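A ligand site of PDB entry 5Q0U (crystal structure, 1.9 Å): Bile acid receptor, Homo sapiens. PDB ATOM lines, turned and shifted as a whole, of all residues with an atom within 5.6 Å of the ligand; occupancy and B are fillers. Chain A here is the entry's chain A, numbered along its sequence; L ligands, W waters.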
ATOM      1  N   GLN A  24      16.701  33.133  21.719  1.00  0.00           N
ATOM      2  CA  GLN A  24      16.309  31.811  21.206  1.00  0.00           C
ATOM      3  C   GLN A  24      17.092  31.421  19.978  1.00  0.00           C
ATOM      4  O   GLN A  24      17.768  32.267  19.385  1.00  0.00           O
ATOM      5  CB  GLN A  24      14.838  31.828  20.824  1.00  0.00           C
ATOM      6  CG  GLN A  24      13.932  32.075  21.994  1.00  0.00           C
ATOM      7  CD  GLN A  24      12.524  32.090  21.545  1.00  0.00           C
ATOM      8  OE1 GLN A  24      11.748  31.231  21.947  1.00  0.00           O
ATOM      9  NE2 GLN A  24      12.175  33.056  20.681  1.00  0.00           N
ATOM     10  N   ARG A  25      16.991  30.140  19.555  1.00  0.00           N
ATOM     11  CA  ARG A  25      17.684  29.659  18.345  1.00  0.00           C
ATOM     12  C   ARG A  25      17.058  30.345  17.127  1.00  0.00           C
ATOM     13  O   ARG A  25      15.883  30.729  17.171  1.00  0.00           O
ATOM     14  CB  ARG A  25      17.559  28.127  18.206  1.00  0.00           C
ATOM     15  CG  ARG A  25      18.493  27.372  19.135  1.00  0.00           C
ATOM     16  CD  ARG A  25      18.411  25.872  18.918  1.00  0.00           C
ATOM     17  NE  ARG A  25      19.341  25.167  19.794  1.00  0.00           N
ATOM     18  CZ  ARG A  25      19.203  23.893  20.169  1.00  0.00           C
ATOM     19  NH1 ARG A  25      18.163  23.183  19.733  1.00  0.00           N
ATOM     20  NH2 ARG A  25      20.086  23.334  20.971  1.00  0.00           N
ATOM     21  N   MET A  26      17.829  30.528  16.077  1.00  0.00           N
ATOM     22  CA  MET A  26      17.341  31.189  14.874  1.00  0.00           C
ATOM     23  C   MET A  26      16.349  30.272  14.129  1.00  0.00           C
ATOM     24  O   MET A  26      16.626  29.080  14.008  1.00  0.00           O
ATOM     25  CB  MET A  26      18.525  31.570  13.971  1.00  0.00           C
ATOM     26  CG  MET A  26      18.257  32.769  13.091  1.00  0.00           C
ATOM     27  SD  MET A  26      18.093  34.318  14.021  1.00  0.00           S
ATOM     28  CE  MET A  26      16.821  35.155  13.024  1.00  0.00           C
ATOM     29  N   ILE A  30      16.639  25.865  12.519  1.00  0.00           N
ATOM     30  CA  ILE A  30      15.630  24.841  12.736  1.00  0.00           C
ATOM     31  C   ILE A  30      15.069  24.300  11.398  1.00  0.00           C
ATOM     32  O   ILE A  30      15.027  23.078  11.198  1.00  0.00           O
ATOM     33  CB  ILE A  30      14.528  25.444  13.671  1.00  0.00           C
ATOM     34  CG1 ILE A  30      15.165  25.977  15.010  1.00  0.00           C
ATOM     35  CG2 ILE A  30      13.380  24.467  13.927  1.00  0.00           C
ATOM     36  CD1 ILE A  30      14.652  27.100  15.512  1.00  0.00           C
ATOM     37  N   THR A  31      14.639  25.217  10.501  1.00  0.00           N
ATOM     38  CA  THR A  31      14.030  24.863   9.220  1.00  0.00           C
ATOM     39  C   THR A  31      15.039  24.318   8.217  1.00  0.00           C
ATOM     40  O   THR A  31      14.674  23.439   7.429  1.00  0.00           O
ATOM     41  CB  THR A  31      13.208  26.013   8.638  1.00  0.00           C
ATOM     42  OG1 THR A  31      14.024  27.171   8.567  1.00  0.00           O
ATOM     43  CG2 THR A  31      11.942  26.293   9.442  1.00  0.00           C
ATOM     44  N   ILE A  34      15.386  20.538   8.948  1.00  0.00           N
ATOM     45  CA  ILE A  34      14.201  19.790   8.493  1.00  0.00           C
ATOM     46  C   ILE A  34      14.160  19.733   6.942  1.00  0.00           C
ATOM     47  O   ILE A  34      13.820  18.692   6.394  1.00  0.00           O
ATOM     48  CB  ILE A  34      12.893  20.394   9.104  1.00  0.00           C
ATOM     49  CG1 ILE A  34      12.916  20.386  10.661  1.00  0.00           C
ATOM     50  CG2 ILE A  34      11.632  19.698   8.566  1.00  0.00           C
ATOM     51  CD1 ILE A  34      11.802  21.322  11.363  1.00  0.00           C
ATOM     52  N   ASN A  44      13.630  12.014  14.004  1.00  0.00           N
ATOM     53  CA  ASN A  44      12.822  13.202  14.281  1.00  0.00           C
ATOM     54  C   ASN A  44      12.410  13.305  15.759  1.00  0.00           C
ATOM     55  O   ASN A  44      12.370  14.397  16.316  1.00  0.00           O
ATOM     56  CB  ASN A  44      11.597  13.255  13.366  1.00  0.00           C
ATOM     57  CG  ASN A  44      11.924  13.734  11.983  1.00  0.00           C
ATOM     58  OD1 ASN A  44      12.740  14.638  11.782  1.00  0.00           O
ATOM     59  ND2 ASN A  44      11.255  13.154  10.992  1.00  0.00           N
ATOM     60  N   ILE A  47      15.404  14.727  17.509  1.00  0.00           N
ATOM     61  CA  ILE A  47      15.523  16.163  17.180  1.00  0.00           C
ATOM     62  C   ILE A  47      14.521  16.922  18.059  1.00  0.00           C
ATOM     63  O   ILE A  47      14.874  17.929  18.651  1.00  0.00           O
ATOM     64  CB  ILE A  47      15.304  16.419  15.646  1.00  0.00           C
ATOM     65  CG1 ILE A  47      16.515  15.895  14.823  1.00  0.00           C
ATOM     66  CG2 ILE A  47      15.043  17.913  15.339  1.00  0.00           C
ATOM     67  CD1 ILE A  47      16.227  15.664  13.297  1.00  0.00           C
ATOM     68  N   LEU A  48      13.270  16.406  18.153  1.00  0.00           N
ATOM     69  CA  LEU A  48      12.230  17.042  18.966  1.00  0.00           C
ATOM     70  C   LEU A  48      12.626  17.160  20.445  1.00  0.00           C
ATOM     71  O   LEU A  48      12.471  18.237  21.009  1.00  0.00           O
ATOM     72  CB  LEU A  48      10.908  16.240  18.845  1.00  0.00           C
ATOM     73  CG  LEU A  48       9.762  16.591  19.847  1.00  0.00           C
ATOM     74  CD1 LEU A  48       9.219  17.992  19.617  1.00  0.00           C
ATOM     75  CD2 LEU A  48       8.651  15.583  19.766  1.00  0.00           C
ATOM     76  N   MET A  51      15.477  19.751  20.809  1.00  0.00           N
ATOM     77  CA  MET A  51      14.914  21.095  20.573  1.00  0.00           C
ATOM     78  C   MET A  51      14.044  21.557  21.740  1.00  0.00           C
ATOM     79  O   MET A  51      14.109  22.714  22.122  1.00  0.00           O
ATOM     80  CB  MET A  51      14.103  21.145  19.260  1.00  0.00           C
ATOM     81  CG  MET A  51      14.935  20.964  18.031  1.00  0.00           C
ATOM     82  SD  MET A  51      15.699  22.503  17.589  1.00  0.00           S
ATOM     83  CE  MET A  51      17.159  21.891  16.687  1.00  0.00           C
ATOM     84  N   ALA A  52      13.176  20.662  22.250  1.00  0.00           N
ATOM     85  CA  ALA A  52      12.261  20.979  23.330  1.00  0.00           C
ATOM     86  C   ALA A  52      12.980  21.171  24.657  1.00  0.00           C
ATOM     87  O   ALA A  52      12.512  21.983  25.442  1.00  0.00           O
ATOM     88  CB  ALA A  52      11.194  19.916  23.467  1.00  0.00           C
ATOM     89  N   ASN A  54      16.139  22.317  24.955  1.00  0.00           N
ATOM     90  CA  ASN A  54      16.775  23.632  24.820  1.00  0.00           C
ATOM     91  C   ASN A  54      15.709  24.753  24.980  1.00  0.00           C
ATOM     92  O   ASN A  54      15.995  25.740  25.644  1.00  0.00           O
ATOM     93  CB  ASN A  54      17.552  23.774  23.515  1.00  0.00           C
ATOM     94  CG  ASN A  54      18.138  25.164  23.340  1.00  0.00           C
ATOM     95  OD1 ASN A  54      17.639  25.977  22.549  1.00  0.00           O
ATOM     96  ND2 ASN A  54      19.137  25.514  24.151  1.00  0.00           N
ATOM     97  N   HIS A  55      14.508  24.593  24.374  1.00  0.00           N
ATOM     98  CA  HIS A  55      13.447  25.594  24.497  1.00  0.00           C
ATOM     99  C   HIS A  55      13.078  25.827  25.970  1.00  0.00           C
ATOM    100  O   HIS A  55      12.866  26.986  26.368  1.00  0.00           O
ATOM    101  CB  HIS A  55      12.215  25.220  23.665  1.00  0.00           C
ATOM    102  CG  HIS A  55      11.128  26.240  23.769  1.00  0.00           C
ATOM    103  ND1 HIS A  55      10.063  26.073  24.623  1.00  0.00           N
ATOM    104  CD2 HIS A  55      11.021  27.456  23.172  1.00  0.00           C
ATOM    105  CE1 HIS A  55       9.333  27.177  24.519  1.00  0.00           C
ATOM    106  NE2 HIS A  55       9.862  28.029  23.628  1.00  0.00           N
ATOM    107  N   VAL A  58      15.690  28.074  27.527  1.00  0.00           N
ATOM    108  CA  VAL A  58      15.551  29.436  27.003  1.00  0.00           C
ATOM    109  C   VAL A  58      14.299  30.115  27.600  1.00  0.00           C
ATOM    110  O   VAL A  58      14.342  31.292  27.948  1.00  0.00           O
ATOM    111  CB  VAL A  58      15.503  29.400  25.457  1.00  0.00           C
ATOM    112  CG1 VAL A  58      15.198  30.764  24.916  1.00  0.00           C
ATOM    113  CG2 VAL A  58      16.854  28.919  24.895  1.00  0.00           C
ATOM    114  N   MET A  89       6.035  26.522  23.653  1.00  0.00           N
ATOM    115  CA  MET A  89       6.754  25.722  22.650  1.00  0.00           C
ATOM    116  C   MET A  89       5.943  25.630  21.344  1.00  0.00           C
ATOM    117  O   MET A  89       6.528  25.785  20.272  1.00  0.00           O
ATOM    118  CB  MET A  89       7.065  24.351  23.251  1.00  0.00           C
ATOM    119  CG  MET A  89       8.064  23.541  22.483  1.00  0.00           C
ATOM    120  SD  MET A  89       7.217  22.531  21.259  1.00  0.00           S
ATOM    121  CE  MET A  89       6.248  21.399  22.322  1.00  0.00           C
ATOM    122  N   PHE A  90       4.605  25.498  21.425  1.00  0.00           N
ATOM    123  CA  PHE A  90       3.757  25.452  20.243  1.00  0.00           C
ATOM    124  C   PHE A  90       3.617  26.807  19.600  1.00  0.00           C
ATOM    125  O   PHE A  90       3.513  26.893  18.387  1.00  0.00           O
ATOM    126  CB  PHE A  90       2.369  24.847  20.526  1.00  0.00           C
ATOM    127  CG  PHE A  90       2.415  23.333  20.531  1.00  0.00           C
ATOM    128  CD1 PHE A  90       2.679  22.630  19.360  1.00  0.00           C
ATOM    129  CD2 PHE A  90       2.230  22.625  21.711  1.00  0.00           C
ATOM    130  CE1 PHE A  90       2.752  21.238  19.374  1.00  0.00           C
ATOM    131  CE2 PHE A  90       2.319  21.228  21.711  1.00  0.00           C
ATOM    132  CZ  PHE A  90       2.564  20.551  20.542  1.00  0.00           C
ATOM    133  N   ARG A  92       5.940  29.143  19.668  1.00  0.00           N
ATOM    134  CA  ARG A  92       7.226  29.338  19.006  1.00  0.00           C
ATOM    135  C   ARG A  92       7.299  28.473  17.719  1.00  0.00           C
ATOM    136  O   ARG A  92       7.772  28.939  16.686  1.00  0.00           O
ATOM    137  CB  ARG A  92       8.397  29.040  19.967  1.00  0.00           C
ATOM    138  CG  ARG A  92       9.772  29.143  19.312  1.00  0.00           C
ATOM    139  CD  ARG A  92      10.088  30.530  18.762  1.00  0.00           C
ATOM    140  NE  ARG A  92      11.473  30.590  18.287  1.00  0.00           N
ATOM    141  CZ  ARG A  92      11.970  31.566  17.563  1.00  0.00           C
ATOM    142  NH1 ARG A  92      11.209  32.591  17.212  1.00  0.00           N
ATOM    143  NH2 ARG A  92      13.244  31.560  17.214  1.00  0.00           N
ATOM    144  N   SER A  93       6.789  27.224  17.767  1.00  0.00           N
ATOM    145  CA  SER A  93       6.760  26.393  16.539  1.00  0.00           C
ATOM    146  C   SER A  93       5.867  27.052  15.476  1.00  0.00           C
ATOM    147  O   SER A  93       6.199  27.006  14.289  1.00  0.00           O
ATOM    148  CB  SER A  93       6.247  25.000  16.850  1.00  0.00           C
ATOM    149  OG  SER A  93       7.129  24.334  17.739  1.00  0.00           O
ATOM    150  N   ALA A  94       4.743  27.664  15.900  1.00  0.00           N
ATOM    151  CA  ALA A  94       3.831  28.342  14.957  1.00  0.00           C
ATOM    152  C   ALA A  94       4.531  29.544  14.336  1.00  0.00           C
ATOM    153  O   ALA A  94       4.382  29.790  13.141  1.00  0.00           O
ATOM    154  CB  ALA A  94       2.557  28.777  15.680  1.00  0.00           C
ATOM    155  N   ILE A  96       7.832  29.926  13.824  1.00  0.00           N
ATOM    156  CA  ILE A  96       8.825  29.379  12.887  1.00  0.00           C
ATOM    157  C   ILE A  96       8.120  28.869  11.646  1.00  0.00           C
ATOM    158  O   ILE A  96       8.539  29.176  10.536  1.00  0.00           O
ATOM    159  CB  ILE A  96       9.695  28.282  13.584  1.00  0.00           C
ATOM    160  CG1 ILE A  96      10.529  28.873  14.723  1.00  0.00           C
ATOM    161  CG2 ILE A  96      10.607  27.559  12.582  1.00  0.00           C
ATOM    162  CD1 ILE A  96      11.036  27.881  15.756  1.00  0.00           C
ATOM    163  N   PHE A  97       6.997  28.149  11.824  1.00  0.00           N
ATOM    164  CA  PHE A  97       6.221  27.641  10.684  1.00  0.00           C
ATOM    165  C   PHE A  97       5.806  28.723   9.699  1.00  0.00           C
ATOM    166  O   PHE A  97       5.829  28.485   8.487  1.00  0.00           O
ATOM    167  CB  PHE A  97       4.976  26.882  11.171  1.00  0.00           C
ATOM    168  CG  PHE A  97       4.239  26.134  10.076  1.00  0.00           C
ATOM    169  CD1 PHE A  97       4.718  24.931   9.581  1.00  0.00           C
ATOM    170  CD2 PHE A  97       3.069  26.657   9.524  1.00  0.00           C
ATOM    171  CE1 PHE A  97       4.042  24.258   8.562  1.00  0.00           C
ATOM    172  CE2 PHE A  97       2.378  25.976   8.519  1.00  0.00           C
ATOM    173  CZ  PHE A  97       2.864  24.780   8.044  1.00  0.00           C
ATOM    174  N   ASN A  98       5.418  29.890  10.209  1.00  0.00           N
ATOM    175  CA  ASN A  98       4.901  30.993   9.391  1.00  0.00           C
ATOM    176  C   ASN A  98       5.950  32.014   8.928  1.00  0.00           C
ATOM    177  O   ASN A  98       5.561  33.025   8.334  1.00  0.00           O
ATOM    178  CB  ASN A  98       3.747  31.699  10.113  1.00  0.00           C
ATOM    179  CG  ASN A  98       2.561  30.784  10.213  1.00  0.00           C
ATOM    180  OD1 ASN A  98       1.915  30.454   9.215  1.00  0.00           O
ATOM    181  ND2 ASN A  98       2.272  30.345  11.416  1.00  0.00           N
ATOM    182  N   LEU A 109       8.408  21.934   4.137  1.00  0.00           N
ATOM    183  CA  LEU A 109       8.469  21.993   5.604  1.00  0.00           C
ATOM    184  C   LEU A 109       7.235  21.334   6.221  1.00  0.00           C
ATOM    185  O   LEU A 109       7.378  20.473   7.085  1.00  0.00           O
ATOM    186  CB  LEU A 109       8.623  23.440   6.092  1.00  0.00           C
ATOM    187  CG  LEU A 109       8.715  23.649   7.617  1.00  0.00           C
ATOM    188  CD1 LEU A 109      10.008  23.044   8.185  1.00  0.00           C
ATOM    189  CD2 LEU A 109       8.582  25.091   7.970  1.00  0.00           C
ATOM    190  N   ARG A 112       7.236  17.517   5.571  1.00  0.00           N
ATOM    191  CA  ARG A 112       8.230  16.887   6.440  1.00  0.00           C
ATOM    192  C   ARG A 112       7.703  16.755   7.871  1.00  0.00           C
ATOM    193  O   ARG A 112       7.903  15.709   8.472  1.00  0.00           O
ATOM    194  CB  ARG A 112       9.544  17.676   6.422  1.00  0.00           C
ATOM    195  CG  ARG A 112      10.337  17.529   5.120  1.00  0.00           C
ATOM    196  CD  ARG A 112      11.372  16.419   5.119  1.00  0.00           C
ATOM    197  NE  ARG A 112      12.359  16.660   4.064  1.00  0.00           N
ATOM    198  CZ  ARG A 112      12.333  16.127   2.844  1.00  0.00           C
ATOM    199  NH1 ARG A 112      11.358  15.301   2.504  1.00  0.00           N
ATOM    200  NH2 ARG A 112      13.277  16.427   1.969  1.00  0.00           N
ATOM    201  N   ILE A 113       7.013  17.780   8.400  1.00  0.00           N
ATOM    202  CA  ILE A 113       6.424  17.750   9.759  1.00  0.00           C
ATOM    203  C   ILE A 113       5.291  16.733   9.792  1.00  0.00           C
ATOM    204  O   ILE A 113       5.232  15.950  10.721  1.00  0.00           O
ATOM    205  CB  ILE A 113       6.015  19.185  10.247  1.00  0.00           C
ATOM    206  CG1 ILE A 113       7.253  20.095  10.368  1.00  0.00           C
ATOM    207  CG2 ILE A 113       5.263  19.144  11.590  1.00  0.00           C
ATOM    208  CD1 ILE A 113       6.947  21.548  10.340  1.00  0.00           C
ATOM    209  N   SER A 116       6.747  13.326  10.136  1.00  0.00           N
ATOM    210  CA  SER A 116       7.788  13.252  11.172  1.00  0.00           C
ATOM    211  C   SER A 116       7.693  12.069  12.155  1.00  0.00           C
ATOM    212  O   SER A 116       8.677  11.738  12.803  1.00  0.00           O
ATOM    213  CB  SER A 116       7.864  14.564  11.947  1.00  0.00           C
ATOM    214  OG  SER A 116       6.664  14.778  12.671  1.00  0.00           O
ATOM    215  N   ILE A 118       4.650  11.845  14.196  1.00  0.00           N
ATOM    216  CA  ILE A 118       3.466  12.237  14.963  1.00  0.00           C
ATOM    217  C   ILE A 118       2.185  11.589  14.374  1.00  0.00           C
ATOM    218  O   ILE A 118       2.097  11.428  13.148  1.00  0.00           O
ATOM    219  CB  ILE A 118       3.386  13.777  14.987  1.00  0.00           C
ATOM    220  CG1 ILE A 118       2.215  14.268  15.843  1.00  0.00           C
ATOM    221  CG2 ILE A 118       3.352  14.379  13.578  1.00  0.00           C
ATOM    222  CD1 ILE A 118       2.607  15.340  16.754  1.00  0.00           C
ATOM    223  N   MET A 126      -2.971  20.631  14.952  1.00  0.00           N
ATOM    224  CA  MET A 126      -1.692  21.346  14.995  1.00  0.00           C
ATOM    225  C   MET A 126      -1.547  22.300  13.823  1.00  0.00           C
ATOM    226  O   MET A 126      -1.227  23.470  14.036  1.00  0.00           O
ATOM    227  CB  MET A 126      -0.533  20.344  15.040  1.00  0.00           C
ATOM    228  CG  MET A 126       0.784  20.975  15.399  1.00  0.00           C
ATOM    229  SD  MET A 126       2.159  19.826  15.237  1.00  0.00           S
ATOM    230  CE  MET A 126       2.071  19.405  13.589  1.00  0.00           C
ATOM    231  N   TYR A 130      -1.399  26.445  13.531  1.00  0.00           N
ATOM    232  CA  TYR A 130      -0.291  27.125  12.836  1.00  0.00           C
ATOM    233  C   TYR A 130      -0.794  27.996  11.700  1.00  0.00           C
ATOM    234  O   TYR A 130      -0.254  29.079  11.477  1.00  0.00           O
ATOM    235  CB  TYR A 130       0.705  26.108  12.228  1.00  0.00           C
ATOM    236  CG  TYR A 130       1.480  25.271  13.205  1.00  0.00           C
ATOM    237  CD1 TYR A 130       1.464  25.545  14.569  1.00  0.00           C
ATOM    238  CD2 TYR A 130       2.280  24.218  12.769  1.00  0.00           C
ATOM    239  CE1 TYR A 130       2.219  24.813  15.478  1.00  0.00           C
ATOM    240  CE2 TYR A 130       3.042  23.466  13.673  1.00  0.00           C
ATOM    241  CZ  TYR A 130       2.999  23.759  15.019  1.00  0.00           C
ATOM    242  OH  TYR A 130       3.703  23.002  15.921  1.00  0.00           O
ATOM    243  N   MET A 211       0.349  13.098  22.546  1.00  0.00           N
ATOM    244  CA  MET A 211       0.979  13.492  21.277  1.00  0.00           C
ATOM    245  C   MET A 211       2.384  12.899  21.177  1.00  0.00           C
ATOM    246  O   MET A 211       2.749  12.357  20.135  1.00  0.00           O
ATOM    247  CB  MET A 211       1.113  15.027  21.168  1.00  0.00           C
ATOM    248  CG  MET A 211      -0.057  15.712  20.555  1.00  0.00           C
ATOM    249  SD  MET A 211       0.367  17.426  20.105  1.00  0.00           S
ATOM    250  CE  MET A 211      -0.166  18.265  21.540  1.00  0.00           C
ATOM    251  N   LEU A 212       3.170  13.033  22.263  1.00  0.00           N
ATOM    252  CA  LEU A 212       4.541  12.535  22.347  1.00  0.00           C
ATOM    253  C   LEU A 212       4.624  11.016  22.426  1.00  0.00           C
ATOM    254  O   LEU A 212       5.466  10.422  21.755  1.00  0.00           O
ATOM    255  CB  LEU A 212       5.252  13.131  23.539  1.00  0.00           C
ATOM    256  CG  LEU A 212       5.236  14.640  23.601  1.00  0.00           C
ATOM    257  CD1 LEU A 212       5.288  15.088  25.015  1.00  0.00           C
ATOM    258  CD2 LEU A 212       6.327  15.234  22.728  1.00  0.00           C
ATOM    259  N   TRP A 215       3.990   9.057  19.163  1.00  0.00           N
ATOM    260  CA  TRP A 215       4.970   9.212  18.092  1.00  0.00           C
ATOM    261  C   TRP A 215       5.368   7.811  17.627  1.00  0.00           C
ATOM    262  O   TRP A 215       5.598   6.943  18.482  1.00  0.00           O
ATOM    263  CB  TRP A 215       6.197   9.949  18.617  1.00  0.00           C
ATOM    264  CG  TRP A 215       6.975  10.664  17.546  1.00  0.00           C
ATOM    265  CD1 TRP A 215       7.901  10.126  16.706  1.00  0.00           C
ATOM    266  CD2 TRP A 215       6.908  12.050  17.248  1.00  0.00           C
ATOM    267  NE1 TRP A 215       8.436  11.112  15.909  1.00  0.00           N
ATOM    268  CE2 TRP A 215       7.821  12.307  16.204  1.00  0.00           C
ATOM    269  CE3 TRP A 215       6.143  13.126  17.759  1.00  0.00           C
ATOM    270  CZ2 TRP A 215       8.018  13.579  15.670  1.00  0.00           C
ATOM    271  CZ3 TRP A 215       6.329  14.384  17.210  1.00  0.00           C
ATOM    272  CH2 TRP A 215       7.245  14.605  16.178  1.00  0.00           C
HETATM  273  C1  LIG L   1      10.695  18.520  15.817  1.00  0.00           C
HETATM  274  C2  LIG L   1       9.868  19.628  15.160  1.00  0.00           C
HETATM  275  C3  LIG L   1       8.784  18.989  14.269  1.00  0.00           C
HETATM  276  C4  LIG L   1       9.268  20.599  16.197  1.00  0.00           C
HETATM  277  C5  LIG L   1      10.298  21.447  16.979  1.00  0.00           C
HETATM  278  C6  LIG L   1       6.848  21.286  15.820  1.00  0.00           C
HETATM  279  C7  LIG L   1       7.942  24.221  12.614  1.00  0.00           C
HETATM  280  C8  LIG L   1       9.444  22.838  13.880  1.00  0.00           C
HETATM  281  C9  LIG L   1       5.515  19.279  16.451  1.00  0.00           C
HETATM  282  C10 LIG L   1       5.010  18.407  17.401  1.00  0.00           C
HETATM  283  C11 LIG L   1       5.291  18.631  18.735  1.00  0.00           C
HETATM  284  C12 LIG L   1       6.574  20.563  18.191  1.00  0.00           C
HETATM  285  C13 LIG L   1       9.374  18.031  13.201  1.00  0.00           C
HETATM  286  C14 LIG L   1      10.275  16.943  13.858  1.00  0.00           C
HETATM  287  C15 LIG L   1      11.342  17.581  14.751  1.00  0.00           C
HETATM  288  O1  LIG L   1      11.431  21.038  17.132  1.00  0.00           O
HETATM  289  N1  LIG L   1       9.883  22.634  17.471  1.00  0.00           N
HETATM  290  C16 LIG L   1      10.787  23.494  18.229  1.00  0.00           C
HETATM  291  C17 LIG L   1      10.059  24.429  19.180  1.00  0.00           C
HETATM  292  C18 LIG L   1      11.055  25.217  20.047  1.00  0.00           C
HETATM  293  C19 LIG L   1      12.088  25.971  19.176  1.00  0.00           C
HETATM  294  C20 LIG L   1      12.789  25.021  18.171  1.00  0.00           C
HETATM  295  C21 LIG L   1      11.753  24.264  17.336  1.00  0.00           C
HETATM  296  O2  LIG L   1      13.125  26.486  20.077  1.00  0.00           O
HETATM  297  S1  LIG L   1      13.717  28.059  20.098  1.00  0.00           S
HETATM  298  O3  LIG L   1      15.097  27.887  20.329  1.00  0.00           O
HETATM  299  O4  LIG L   1      13.429  28.629  18.740  1.00  0.00           O
HETATM  300  O5  LIG L   1      12.907  28.661  21.098  1.00  0.00           O
HETATM  301  N2  LIG L   1       8.202  21.413  15.552  1.00  0.00           N
HETATM  302  C22 LIG L   1       8.335  22.350  14.537  1.00  0.00           C
HETATM  303  C23 LIG L   1       7.038  22.756  14.249  1.00  0.00           C
HETATM  304  N3  LIG L   1       6.115  22.082  15.060  1.00  0.00           N
HETATM  305  C24 LIG L   1       6.300  20.368  16.823  1.00  0.00           C
HETATM  306  C25 LIG L   1       6.069  19.691  19.140  1.00  0.00           C
HETATM  307 CL1  LIG L   1       4.653  17.528  19.932  1.00  0.00          CL
HETATM  308  C26 LIG L   1       6.827  23.732  13.264  1.00  0.00           C
HETATM  309  C27 LIG L   1       9.208  23.792  12.918  1.00  0.00           C
HETATM  310  F1  LIG L   1      10.249  24.317  12.251  1.00  0.00           F
HETATM  311  F2  LIG L   1       7.796  25.159  11.656  1.00  0.00           F
HETATM  312  O   HOH W   1      15.441  24.788  20.945  1.00  0.00           O
HETATM  313  O   HOH W   2      13.917  21.359  14.839  1.00  0.00           O
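The side-chain hydroxyl of Tyr 130 sits at hydrogen-bond distance from a nitrogen (N3) of the ligand (2.7 Å).
The guanidinium group (NE) of Arg 92 lies within salt-bridge range of an oxygen (O4) of the ligand (2.8 Å).
The side-chain hydroxyl (OG) of Ser 93 sits at hydrogen-bond distance from a nitrogen (N1) of the ligand.
The backbone NH (N) of Arg 25 is in hydrogen-bond range of an oxygen (O3) of the ligand, at 3.0 Å.
O5 of the ligand lies close to OE1 of Gln 24 (2.9 Å).
The backbone carbonyl oxygen (O) of Arg 25 lies within hydrogen-bond range of the guanidinium group (NH2) of Arg 92 (2.8 Å).
SD of Met 51 sits at hydrogen-bond distance from NH1 of Arg 25, at 3.3 Å.
The backbone carbonyl oxygen (O) of Ile 34 sits at hydrogen-bond distance from the guanidinium group (NE) of Arg 112 (3.4 Å).
The backbone carbonyl oxygen (O) of Met 89 is in hydrogen-bond range of the side-chain hydroxyl (OG) of Ser 93 (3.0 Å).
The side-chain amide nitrogen (ND2) of Asn 98 lies within hydrogen-bond range of the backbone carbonyl oxygen (O) of Tyr 130, at 2.8 Å.
The side-chain amide oxygen (OD1) of Asn 54 sits at hydrogen-bond distance from the guanidinium group (NE) of Arg 25 (3.3 Å).
OH of Tyr 130 lies close to SD of Met 126 (3.6 Å).
The side-chain amide nitrogen (ND2) of Asn 44 lies close to the backbone carbonyl oxygen (O) of Ser 116, 3.5 Å away.
The backbone NH of Phe 97 lies close to a fluorine (F2) of the ligand (3.1 Å).
Merely in contact with the ligand: Ile 30, Thr 31, Ile 34, Asn 44, Ile 47, Leu 48, Met 51, Asn 54, His 55, Met 89, Phe 90, Ile 96, Leu 109, Ile 113, Ser 116, Ile 118, Met 126 and Leu 212.
Hydrophobic or aromatic side chains within 4 Å of the ligand: Ile 30, Ile 34, Ile 47, Leu 48, Met 51, His 55, Met 89, Phe 90, Ile 96, Phe 97, Leu 109, Ile 113, Ile 118, Met 126, Tyr 130 and Leu 212.
The nearest printed residue that does not touch the ligand is Trp 215 (4.2 Å).
Water W2 bridges O1 of the ligand (3.4 Å) and SD of Met 51 (3.5 Å).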
